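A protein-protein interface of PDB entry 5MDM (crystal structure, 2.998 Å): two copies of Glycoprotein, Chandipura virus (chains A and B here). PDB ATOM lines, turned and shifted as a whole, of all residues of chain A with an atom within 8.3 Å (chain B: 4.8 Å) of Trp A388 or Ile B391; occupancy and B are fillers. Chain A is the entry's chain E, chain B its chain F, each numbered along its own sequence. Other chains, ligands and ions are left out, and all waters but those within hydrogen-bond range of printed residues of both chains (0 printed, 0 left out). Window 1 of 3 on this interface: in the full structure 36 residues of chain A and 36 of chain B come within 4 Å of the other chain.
Among the printed residues, merely in contact across the chains: Trp A388 with Pro B341, Met A393 with Trp B388, Met A393 with Pro B341, Trp A388 with Leu B2, Trp A388 with Ile B391 and Trp A388 with Met B393.
Trp A388 touches just these residues of chain B: Leu B2, Pro B341, Ile B391 and Met B393.
Of chain A, only Trp A388 (3.8 Å) comes within 4 Å of Ile B391.
No residue of chain A comes within 4 Å of Gly B392.
Of the printed residues of chain B, Met A393 touches Pro B341 and Trp B388.
Of the printed residues of chain A, Leu B2 touches Trp A388 (3.6 Å).
Of the printed residues of chain A, Met B393 touches Trp A388 (3.9 Å).
Ser B3 touches none of the printed residues of chain A.
The nearest printed residue of chain A that does not touch Pro B341 is Tyr A1 (4.1 Å).
Of the 12 printed residues of chain B, 5 touch a printed residue of chain A.
Printed residues of chain B that touch a printed residue of chain A: Leu B2, Pro B341, Trp B388, Ile B391 and Met B393.
Of the 23 printed residues of chain A, 2 touch a printed residue of chain B.
Hydrophobic or aromatic side chains of chain A within 4 Å of the printed part of chain B: Trp A388 and Met A393.
Among the printed residues, no Asp or Glu carboxylate lies within 4 Å of a Lys or Arg side-chain nitrogen of the other chain.
Trp A388 touches Leu B2, but with the chains exchanged Leu A2 does not touch Trp B388 (7.5 Å).
Trp A388 touches Ile B391, but with the chains exchanged Ile A391 does not touch Trp B388 (7.6 Å).
Trp A388 touches Met B393, and with the chains exchanged Met A393 touches Trp B388.
Met A393 touches Pro B341, but with the chains exchanged Pro A341 does not touch Met B393 (9.9 Å).
12 positions are printed for both chains.
Of the 6 pairs that touch across the chains among the printed residues, 2 have their exchanged pair printed and touching as well.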
ATOM      1  N   TYR A   1      -0.318  27.858 -23.411  1.00  0.00           N
ATOM      2  CA  TYR A   1       0.984  28.061 -24.035  1.00  0.00           C
ATOM      3  C   TYR A   1       2.074  27.337 -23.248  1.00  0.00           C
ATOM      4  O   TYR A   1       3.159  27.050 -23.770  1.00  0.00           O
ATOM      5  CB  TYR A   1       1.296  29.556 -24.166  1.00  0.00           C
ATOM      6  CG  TYR A   1       1.300  30.320 -22.860  1.00  0.00           C
ATOM      7  CD1 TYR A   1       2.489  30.590 -22.197  1.00  0.00           C
ATOM      8  CD2 TYR A   1       0.115  30.781 -22.296  1.00  0.00           C
ATOM      9  CE1 TYR A   1       2.500  31.294 -21.005  1.00  0.00           C
ATOM     10  CE2 TYR A   1       0.116  31.482 -21.103  1.00  0.00           C
ATOM     11  CZ  TYR A   1       1.312  31.735 -20.461  1.00  0.00           C
ATOM     12  OH  TYR A   1       1.327  32.435 -19.272  1.00  0.00           O
ATOM     13  N   LEU A   2       1.770  27.041 -21.990  1.00  0.00           N
ATOM     14  CA  LEU A   2       2.659  26.263 -21.143  1.00  0.00           C
ATOM     15  C   LEU A   2       2.268  24.793 -21.179  1.00  0.00           C
ATOM     16  O   LEU A   2       1.126  24.435 -20.885  1.00  0.00           O
ATOM     17  CB  LEU A   2       2.585  26.762 -19.706  1.00  0.00           C
ATOM     18  CG  LEU A   2       2.968  28.219 -19.491  1.00  0.00           C
ATOM     19  CD1 LEU A   2       2.910  28.545 -18.018  1.00  0.00           C
ATOM     20  CD2 LEU A   2       4.349  28.486 -20.043  1.00  0.00           C
ATOM     21  N   SER A   3       3.220  23.940 -21.535  1.00  0.00           N
ATOM     22  CA  SER A   3       2.956  22.512 -21.583  1.00  0.00           C
ATOM     23  C   SER A   3       3.844  21.757 -20.613  1.00  0.00           C
ATOM     24  O   SER A   3       4.898  22.238 -20.215  1.00  0.00           O
ATOM     25  CB  SER A   3       3.144  21.983 -23.000  1.00  0.00           C
ATOM     26  OG  SER A   3       4.063  22.797 -23.703  1.00  0.00           O
ATOM     27  N   ILE A   4       3.391  20.577 -20.212  1.00  0.00           N
ATOM     28  CA  ILE A   4       4.180  19.693 -19.376  1.00  0.00           C
ATOM     29  C   ILE A   4       3.923  18.282 -19.846  1.00  0.00           C
ATOM     30  O   ILE A   4       2.937  18.020 -20.541  1.00  0.00           O
ATOM     31  CB  ILE A   4       3.760  19.772 -17.897  1.00  0.00           C
ATOM     32  CG1 ILE A   4       2.267  19.473 -17.753  1.00  0.00           C
ATOM     33  CG2 ILE A   4       4.105  21.128 -17.298  1.00  0.00           C
ATOM     34  CD1 ILE A   4       1.816  19.340 -16.324  1.00  0.00           C
ATOM     35  N   LEU A 303      11.608  19.576  -5.662  1.00  0.00           N
ATOM     36  CA  LEU A 303      12.409  19.892  -6.840  1.00  0.00           C
ATOM     37  C   LEU A 303      13.298  18.707  -7.236  1.00  0.00           C
ATOM     38  O   LEU A 303      13.395  18.334  -8.423  1.00  0.00           O
ATOM     39  CB  LEU A 303      13.254  21.139  -6.573  1.00  0.00           C
ATOM     40  CG  LEU A 303      14.003  21.741  -7.762  1.00  0.00           C
ATOM     41  CD1 LEU A 303      13.079  21.902  -8.961  1.00  0.00           C
ATOM     42  CD2 LEU A 303      14.606  23.079  -7.374  1.00  0.00           C
ATOM     43  N   SER A 306      11.284  16.356  -8.959  1.00  0.00           N
ATOM     44  CA  SER A 306      10.958  16.788 -10.307  1.00  0.00           C
ATOM     45  C   SER A 306      12.099  16.511 -11.269  1.00  0.00           C
ATOM     46  O   SER A 306      11.879  16.373 -12.471  1.00  0.00           O
ATOM     47  CB  SER A 306      10.640  18.272 -10.318  1.00  0.00           C
ATOM     48  OG  SER A 306      11.796  19.033 -10.019  1.00  0.00           O
ATOM     49  N   TYR A 307      13.319  16.433 -10.750  1.00  0.00           N
ATOM     50  CA  TYR A 307      14.449  16.063 -11.608  1.00  0.00           C
ATOM     51  C   TYR A 307      14.359  14.619 -12.119  1.00  0.00           C
ATOM     52  O   TYR A 307      15.133  14.212 -12.982  1.00  0.00           O
ATOM     53  CB  TYR A 307      15.788  16.317 -10.908  1.00  0.00           C
ATOM     54  CG  TYR A 307      16.071  17.787 -10.689  1.00  0.00           C
ATOM     55  CD1 TYR A 307      15.635  18.734 -11.605  1.00  0.00           C
ATOM     56  CD2 TYR A 307      16.750  18.229  -9.562  1.00  0.00           C
ATOM     57  CE1 TYR A 307      15.879  20.079 -11.412  1.00  0.00           C
ATOM     58  CE2 TYR A 307      16.996  19.575  -9.360  1.00  0.00           C
ATOM     59  CZ  TYR A 307      16.558  20.494 -10.289  1.00  0.00           C
ATOM     60  OH  TYR A 307      16.796  21.835 -10.102  1.00  0.00           O
ATOM     61  N   LYS A 311      10.140  14.499 -19.193  1.00  0.00           N
ATOM     62  CA  LYS A 311       9.794  15.785 -19.783  1.00  0.00           C
ATOM     63  C   LYS A 311       9.132  15.620 -21.141  1.00  0.00           C
ATOM     64  O   LYS A 311       8.738  16.598 -21.764  1.00  0.00           O
ATOM     65  CB  LYS A 311      11.017  16.696 -19.890  1.00  0.00           C
ATOM     66  CG  LYS A 311      11.506  17.238 -18.560  1.00  0.00           C
ATOM     67  CD  LYS A 311      12.486  18.374 -18.773  1.00  0.00           C
ATOM     68  CE  LYS A 311      13.006  18.924 -17.457  1.00  0.00           C
ATOM     69  NZ  LYS A 311      13.827  20.150 -17.688  1.00  0.00           N
ATOM     70  N   ILE A 338      -1.112  23.531 -19.260  1.00  0.00           N
ATOM     71  CA  ILE A 338      -1.592  24.095 -18.006  1.00  0.00           C
ATOM     72  C   ILE A 338      -1.630  25.617 -18.081  1.00  0.00           C
ATOM     73  O   ILE A 338      -0.957  26.219 -18.920  1.00  0.00           O
ATOM     74  CB  ILE A 338      -0.731  23.649 -16.820  1.00  0.00           C
ATOM     75  CG1 ILE A 338       0.730  24.034 -17.047  1.00  0.00           C
ATOM     76  CG2 ILE A 338      -0.868  22.151 -16.606  1.00  0.00           C
ATOM     77  CD1 ILE A 338       1.644  23.613 -15.925  1.00  0.00           C
ATOM     78  N   ASP A 339      -2.419  26.231 -17.201  1.00  0.00           N
ATOM     79  CA  ASP A 339      -2.670  27.670 -17.267  1.00  0.00           C
ATOM     80  C   ASP A 339      -1.518  28.523 -16.734  1.00  0.00           C
ATOM     81  O   ASP A 339      -1.429  29.709 -17.041  1.00  0.00           O
ATOM     82  CB  ASP A 339      -3.977  28.028 -16.553  1.00  0.00           C
ATOM     83  CG  ASP A 339      -5.195  27.416 -17.224  1.00  0.00           C
ATOM     84  OD1 ASP A 339      -5.085  26.283 -17.735  1.00  0.00           O
ATOM     85  OD2 ASP A 339      -6.261  28.067 -17.244  1.00  0.00           O
ATOM     86  N   GLY A 340      -0.638  27.917 -15.945  1.00  0.00           N
ATOM     87  CA  GLY A 340       0.508  28.624 -15.397  1.00  0.00           C
ATOM     88  C   GLY A 340       1.318  27.749 -14.462  1.00  0.00           C
ATOM     89  O   GLY A 340       0.858  26.680 -14.063  1.00  0.00           O
ATOM     90  N   PRO A 341       2.532  28.195 -14.099  1.00  0.00           N
ATOM     91  CA  PRO A 341       3.421  27.425 -13.218  1.00  0.00           C
ATOM     92  C   PRO A 341       2.798  27.193 -11.853  1.00  0.00           C
ATOM     93  O   PRO A 341       3.124  26.217 -11.181  1.00  0.00           O
ATOM     94  CB  PRO A 341       4.665  28.312 -13.097  1.00  0.00           C
ATOM     95  CG  PRO A 341       4.209  29.674 -13.479  1.00  0.00           C
ATOM     96  CD  PRO A 341       3.131  29.478 -14.499  1.00  0.00           C
ATOM     97  N   VAL A 342       1.907  28.093 -11.456  1.00  0.00           N
ATOM     98  CA  VAL A 342       1.121  27.914 -10.245  1.00  0.00           C
ATOM     99  C   VAL A 342      -0.363  28.001 -10.601  1.00  0.00           C
ATOM    100  O   VAL A 342      -0.770  28.882 -11.357  1.00  0.00           O
ATOM    101  CB  VAL A 342       1.514  28.947  -9.166  1.00  0.00           C
ATOM    102  CG1 VAL A 342       1.823  30.299  -9.807  1.00  0.00           C
ATOM    103  CG2 VAL A 342       0.434  29.055  -8.092  1.00  0.00           C
ATOM    104  N   LYS A 385       1.631  23.966  -7.385  1.00  0.00           N
ATOM    105  CA  LYS A 385       2.910  24.401  -7.943  1.00  0.00           C
ATOM    106  C   LYS A 385       3.684  23.307  -8.685  1.00  0.00           C
ATOM    107  O   LYS A 385       3.923  22.208  -8.155  1.00  0.00           O
ATOM    108  CB  LYS A 385       3.791  25.013  -6.848  1.00  0.00           C
ATOM    109  CG  LYS A 385       3.147  26.176  -6.105  1.00  0.00           C
ATOM    110  CD  LYS A 385       4.115  26.801  -5.105  1.00  0.00           C
ATOM    111  CE  LYS A 385       3.500  27.999  -4.388  1.00  0.00           C
ATOM    112  NZ  LYS A 385       2.360  27.613  -3.508  1.00  0.00           N
ATOM    113  N   PHE A 386       4.053  23.632  -9.922  1.00  0.00           N
ATOM    114  CA  PHE A 386       4.997  22.850 -10.709  1.00  0.00           C
ATOM    115  C   PHE A 386       6.328  23.581 -10.677  1.00  0.00           C
ATOM    116  O   PHE A 386       6.363  24.813 -10.674  1.00  0.00           O
ATOM    117  CB  PHE A 386       4.545  22.746 -12.170  1.00  0.00           C
ATOM    118  CG  PHE A 386       3.402  21.795 -12.399  1.00  0.00           C
ATOM    119  CD1 PHE A 386       3.627  20.432 -12.505  1.00  0.00           C
ATOM    120  CD2 PHE A 386       2.103  22.268 -12.534  1.00  0.00           C
ATOM    121  CE1 PHE A 386       2.577  19.553 -12.726  1.00  0.00           C
ATOM    122  CE2 PHE A 386       1.051  21.396 -12.754  1.00  0.00           C
ATOM    123  CZ  PHE A 386       1.289  20.036 -12.848  1.00  0.00           C
ATOM    124  N   PRO A 387       7.435  22.827 -10.654  1.00  0.00           N
ATOM    125  CA  PRO A 387       8.762  23.422 -10.826  1.00  0.00           C
ATOM    126  C   PRO A 387       8.906  23.914 -12.260  1.00  0.00           C
ATOM    127  O   PRO A 387       8.518  23.208 -13.190  1.00  0.00           O
ATOM    128  CB  PRO A 387       9.697  22.246 -10.577  1.00  0.00           C
ATOM    129  CG  PRO A 387       8.888  21.060 -10.938  1.00  0.00           C
ATOM    130  CD  PRO A 387       7.502  21.366 -10.495  1.00  0.00           C
ATOM    131  N   TRP A 388       9.460  25.107 -12.439  1.00  0.00           N
ATOM    132  CA  TRP A 388       9.461  25.759 -13.742  1.00  0.00           C
ATOM    133  C   TRP A 388      10.125  24.954 -14.855  1.00  0.00           C
ATOM    134  O   TRP A 388       9.819  25.140 -16.033  1.00  0.00           O
ATOM    135  CB  TRP A 388      10.114  27.138 -13.646  1.00  0.00           C
ATOM    136  CG  TRP A 388      10.053  27.894 -14.931  1.00  0.00           C
ATOM    137  CD1 TRP A 388      11.105  28.297 -15.699  1.00  0.00           C
ATOM    138  CD2 TRP A 388       8.871  28.319 -15.613  1.00  0.00           C
ATOM    139  NE1 TRP A 388      10.651  28.958 -16.813  1.00  0.00           N
ATOM    140  CE2 TRP A 388       9.281  28.984 -16.786  1.00  0.00           C
ATOM    141  CE3 TRP A 388       7.501  28.209 -15.342  1.00  0.00           C
ATOM    142  CZ2 TRP A 388       8.374  29.533 -17.688  1.00  0.00           C
ATOM    143  CZ3 TRP A 388       6.602  28.754 -16.236  1.00  0.00           C
ATOM    144  CH2 TRP A 388       7.041  29.404 -17.395  1.00  0.00           C
ATOM    145  N   HIS A 389      11.030  24.056 -14.488  1.00  0.00           N
ATOM    146  CA  HIS A 389      11.814  23.342 -15.488  1.00  0.00           C
ATOM    147  C   HIS A 389      11.027  22.235 -16.170  1.00  0.00           C
ATOM    148  O   HIS A 389      11.402  21.789 -17.252  1.00  0.00           O
ATOM    149  CB  HIS A 389      13.096  22.784 -14.879  1.00  0.00           C
ATOM    150  CG  HIS A 389      12.883  21.595 -13.998  1.00  0.00           C
ATOM    151  ND1 HIS A 389      13.043  20.300 -14.445  1.00  0.00           N
ATOM    152  CD2 HIS A 389      12.539  21.500 -12.692  1.00  0.00           C
ATOM    153  CE1 HIS A 389      12.802  19.461 -13.454  1.00  0.00           C
ATOM    154  NE2 HIS A 389      12.492  20.163 -12.380  1.00  0.00           N
ATOM    155  N   LEU A 390       9.940  21.798 -15.541  1.00  0.00           N
ATOM    156  CA  LEU A 390       9.086  20.768 -16.114  1.00  0.00           C
ATOM    157  C   LEU A 390       8.173  21.356 -17.174  1.00  0.00           C
ATOM    158  O   LEU A 390       7.529  20.631 -17.936  1.00  0.00           O
ATOM    159  CB  LEU A 390       8.247  20.099 -15.029  1.00  0.00           C
ATOM    160  CG  LEU A 390       9.003  19.160 -14.097  1.00  0.00           C
ATOM    161  CD1 LEU A 390       8.023  18.383 -13.247  1.00  0.00           C
ATOM    162  CD2 LEU A 390       9.903  18.221 -14.886  1.00  0.00           C
ATOM    163  N   ILE A 391       8.129  22.680 -17.216  1.00  0.00           N
ATOM    164  CA  ILE A 391       7.257  23.400 -18.128  1.00  0.00           C
ATOM    165  C   ILE A 391       8.008  23.844 -19.374  1.00  0.00           C
ATOM    166  O   ILE A 391       9.141  24.320 -19.295  1.00  0.00           O
ATOM    167  CB  ILE A 391       6.669  24.635 -17.440  1.00  0.00           C
ATOM    168  CG1 ILE A 391       6.005  24.222 -16.131  1.00  0.00           C
ATOM    169  CG2 ILE A 391       5.703  25.359 -18.361  1.00  0.00           C
ATOM    170  CD1 ILE A 391       5.361  25.357 -15.401  1.00  0.00           C
ATOM    171  N   GLY A 392       7.368  23.684 -20.524  1.00  0.00           N
ATOM    172  CA  GLY A 392       7.926  24.143 -21.778  1.00  0.00           C
ATOM    173  C   GLY A 392       6.995  25.108 -22.481  1.00  0.00           C
ATOM    174  O   GLY A 392       5.785  25.127 -22.231  1.00  0.00           O
ATOM    175  N   MET A 393       7.564  25.908 -23.375  1.00  0.00           N
ATOM    176  CA  MET A 393       6.807  26.910 -24.112  1.00  0.00           C
ATOM    177  C   MET A 393       7.454  27.210 -25.464  1.00  0.00           C
ATOM    178  O   MET A 393       8.678  27.195 -25.596  1.00  0.00           O
ATOM    179  CB  MET A 393       6.719  28.185 -23.278  1.00  0.00           C
ATOM    180  CG  MET A 393       7.980  28.426 -22.463  1.00  0.00           C
ATOM    181  SD  MET A 393       7.822  29.792 -21.314  1.00  0.00           S
ATOM    182  CE  MET A 393       7.435  31.101 -22.464  1.00  0.00           C
ATOM    183  N   LEU A 400       3.309  30.689 -29.000  1.00  0.00           N
ATOM    184  CA  LEU A 400       4.179  31.840 -28.770  1.00  0.00           C
ATOM    185  C   LEU A 400       5.051  32.154 -29.972  1.00  0.00           C
ATOM    186  O   LEU A 400       6.222  32.504 -29.825  1.00  0.00           O
ATOM    187  CB  LEU A 400       5.040  31.632 -27.524  1.00  0.00           C
ATOM    188  CG  LEU A 400       4.253  31.504 -26.218  1.00  0.00           C
ATOM    189  CD1 LEU A 400       5.181  31.183 -25.077  1.00  0.00           C
ATOM    190  CD2 LEU A 400       3.461  32.767 -25.919  1.00  0.00           C
ATOM    191  N   LEU B   2       8.383  33.496 -10.521  1.00  0.00           N
ATOM    192  CA  LEU B   2       9.582  33.358 -11.339  1.00  0.00           C
ATOM    193  C   LEU B   2      10.462  34.583 -11.156  1.00  0.00           C
ATOM    194  O   LEU B   2      10.043  35.700 -11.446  1.00  0.00           O
ATOM    195  CB  LEU B   2       9.221  33.216 -12.817  1.00  0.00           C
ATOM    196  CG  LEU B   2       8.279  32.085 -13.227  1.00  0.00           C
ATOM    197  CD1 LEU B   2       7.908  32.236 -14.687  1.00  0.00           C
ATOM    198  CD2 LEU B   2       8.912  30.726 -12.970  1.00  0.00           C
ATOM    199  N   SER B   3      11.681  34.374 -10.675  1.00  0.00           N
ATOM    200  CA  SER B   3      12.614  35.476 -10.515  1.00  0.00           C
ATOM    201  C   SER B   3      13.258  35.838 -11.848  1.00  0.00           C
ATOM    202  O   SER B   3      13.684  34.965 -12.609  1.00  0.00           O
ATOM    203  CB  SER B   3      13.695  35.120  -9.502  1.00  0.00           C
ATOM    204  OG  SER B   3      14.617  34.207 -10.063  1.00  0.00           O
ATOM    205  N   ILE B   4      13.308  37.131 -12.139  1.00  0.00           N
ATOM    206  CA  ILE B   4      14.022  37.616 -13.308  1.00  0.00           C
ATOM    207  C   ILE B   4      14.860  38.824 -12.940  1.00  0.00           C
ATOM    208  O   ILE B   4      14.807  39.312 -11.816  1.00  0.00           O
ATOM    209  CB  ILE B   4      13.080  38.016 -14.447  1.00  0.00           C
ATOM    210  CG1 ILE B   4      12.185  39.169 -14.007  1.00  0.00           C
ATOM    211  CG2 ILE B   4      12.253  36.825 -14.897  1.00  0.00           C
ATOM    212  CD1 ILE B   4      11.568  39.915 -15.154  1.00  0.00           C
ATOM    213  N   LYS B 311      21.001  38.518 -17.302  1.00  0.00           N
ATOM    214  CA  LYS B 311      20.036  37.647 -16.634  1.00  0.00           C
ATOM    215  C   LYS B 311      20.262  37.637 -15.141  1.00  0.00           C
ATOM    216  O   LYS B 311      19.611  36.890 -14.414  1.00  0.00           O
ATOM    217  CB  LYS B 311      20.120  36.218 -17.160  1.00  0.00           C
ATOM    218  CG  LYS B 311      19.573  36.036 -18.554  1.00  0.00           C
ATOM    219  CD  LYS B 311      19.592  34.578 -18.949  1.00  0.00           C
ATOM    220  CE  LYS B 311      18.818  33.738 -17.969  1.00  0.00           C
ATOM    221  NZ  LYS B 311      18.550  32.398 -18.549  1.00  0.00           N
ATOM    222  N   PRO B 341       5.521  33.874 -17.868  1.00  0.00           N
ATOM    223  CA  PRO B 341       6.114  34.506 -19.053  1.00  0.00           C
ATOM    224  C   PRO B 341       5.112  35.382 -19.801  1.00  0.00           C
ATOM    225  O   PRO B 341       5.520  36.324 -20.481  1.00  0.00           O
ATOM    226  CB  PRO B 341       6.507  33.320 -19.934  1.00  0.00           C
ATOM    227  CG  PRO B 341       6.295  32.106 -19.106  1.00  0.00           C
ATOM    228  CD  PRO B 341       5.275  32.442 -18.081  1.00  0.00           C
ATOM    229  N   PRO B 387      10.379  36.755 -23.441  1.00  0.00           N
ATOM    230  CA  PRO B 387      11.131  35.630 -24.001  1.00  0.00           C
ATOM    231  C   PRO B 387      11.584  34.726 -22.863  1.00  0.00           C
ATOM    232  O   PRO B 387      12.152  35.213 -21.882  1.00  0.00           O
ATOM    233  CB  PRO B 387      12.338  36.306 -24.650  1.00  0.00           C
ATOM    234  CG  PRO B 387      11.895  37.700 -24.923  1.00  0.00           C
ATOM    235  CD  PRO B 387      10.977  38.052 -23.792  1.00  0.00           C
ATOM    236  N   TRP B 388      11.328  33.430 -22.986  1.00  0.00           N
ATOM    237  CA  TRP B 388      11.571  32.504 -21.884  1.00  0.00           C
ATOM    238  C   TRP B 388      13.028  32.433 -21.427  1.00  0.00           C
ATOM    239  O   TRP B 388      13.306  31.996 -20.317  1.00  0.00           O
ATOM    240  CB  TRP B 388      11.043  31.105 -22.220  1.00  0.00           C
ATOM    241  CG  TRP B 388      11.472  30.571 -23.555  1.00  0.00           C
ATOM    242  CD1 TRP B 388      12.617  29.881 -23.837  1.00  0.00           C
ATOM    243  CD2 TRP B 388      10.745  30.659 -24.789  1.00  0.00           C
ATOM    244  NE1 TRP B 388      12.651  29.542 -25.170  1.00  0.00           N
ATOM    245  CE2 TRP B 388      11.514  30.010 -25.775  1.00  0.00           C
ATOM    246  CE3 TRP B 388       9.523  31.232 -25.157  1.00  0.00           C
ATOM    247  CZ2 TRP B 388      11.098  29.917 -27.103  1.00  0.00           C
ATOM    248  CZ3 TRP B 388       9.113  31.140 -26.476  1.00  0.00           C
ATOM    249  CH2 TRP B 388       9.899  30.489 -27.431  1.00  0.00           C
ATOM    250  N   HIS B 389      13.950  32.865 -22.278  1.00  0.00           N
ATOM    251  CA  HIS B 389      15.361  32.896 -21.912  1.00  0.00           C
ATOM    252  C   HIS B 389      15.602  33.715 -20.654  1.00  0.00           C
ATOM    253  O   HIS B 389      16.413  33.345 -19.817  1.00  0.00           O
ATOM    254  CB  HIS B 389      16.202  33.475 -23.044  1.00  0.00           C
ATOM    255  CG  HIS B 389      17.649  33.629 -22.695  1.00  0.00           C
ATOM    256  ND1 HIS B 389      18.272  34.856 -22.627  1.00  0.00           N
ATOM    257  CD2 HIS B 389      18.591  32.708 -22.379  1.00  0.00           C
ATOM    258  CE1 HIS B 389      19.540  34.683 -22.298  1.00  0.00           C
ATOM    259  NE2 HIS B 389      19.758  33.390 -22.137  1.00  0.00           N
ATOM    260  N   LEU B 390      14.884  34.825 -20.529  1.00  0.00           N
ATOM    261  CA  LEU B 390      15.086  35.774 -19.440  1.00  0.00           C
ATOM    262  C   LEU B 390      14.802  35.200 -18.049  1.00  0.00           C
ATOM    263  O   LEU B 390      15.223  35.765 -17.039  1.00  0.00           O
ATOM    264  CB  LEU B 390      14.230  37.017 -19.682  1.00  0.00           C
ATOM    265  CG  LEU B 390      14.574  37.729 -20.990  1.00  0.00           C
ATOM    266  CD1 LEU B 390      13.631  38.897 -21.245  1.00  0.00           C
ATOM    267  CD2 LEU B 390      16.035  38.180 -20.963  1.00  0.00           C
ATOM    268  N   ILE B 391      14.086  34.081 -18.002  1.00  0.00           N
ATOM    269  CA  ILE B 391      13.763  33.426 -16.742  1.00  0.00           C
ATOM    270  C   ILE B 391      14.856  32.430 -16.375  1.00  0.00           C
ATOM    271  O   ILE B 391      15.370  32.437 -15.249  1.00  0.00           O
ATOM    272  CB  ILE B 391      12.416  32.708 -16.833  1.00  0.00           C
ATOM    273  CG1 ILE B 391      11.390  33.618 -17.502  1.00  0.00           C
ATOM    274  CG2 ILE B 391      11.941  32.292 -15.449  1.00  0.00           C
ATOM    275  CD1 ILE B 391      10.051  32.973 -17.700  1.00  0.00           C
ATOM    276  N   GLY B 392      15.191  31.569 -17.332  1.00  0.00           N
ATOM    277  CA  GLY B 392      16.358  30.708 -17.242  1.00  0.00           C
ATOM    278  C   GLY B 392      16.202  29.451 -16.413  1.00  0.00           C
ATOM    279  O   GLY B 392      15.574  28.481 -16.842  1.00  0.00           O
ATOM    280  N   MET B 393      16.795  29.472 -15.222  1.00  0.00           N
ATOM    281  CA  MET B 393      16.774  28.332 -14.312  1.00  0.00           C
ATOM    282  C   MET B 393      15.466  28.285 -13.524  1.00  0.00           C
ATOM    283  O   MET B 393      14.497  27.647 -13.943  1.00  0.00           O
ATOM    284  CB  MET B 393      17.969  28.400 -13.353  1.00  0.00           C
ATOM    285  CG  MET B 393      19.334  28.401 -14.042  1.00  0.00           C
ATOM    286  SD  MET B 393      19.938  26.754 -14.486  1.00  0.00           S
ATOM    287  CE  MET B 393      20.280  26.949 -16.239  1.00  0.00           C
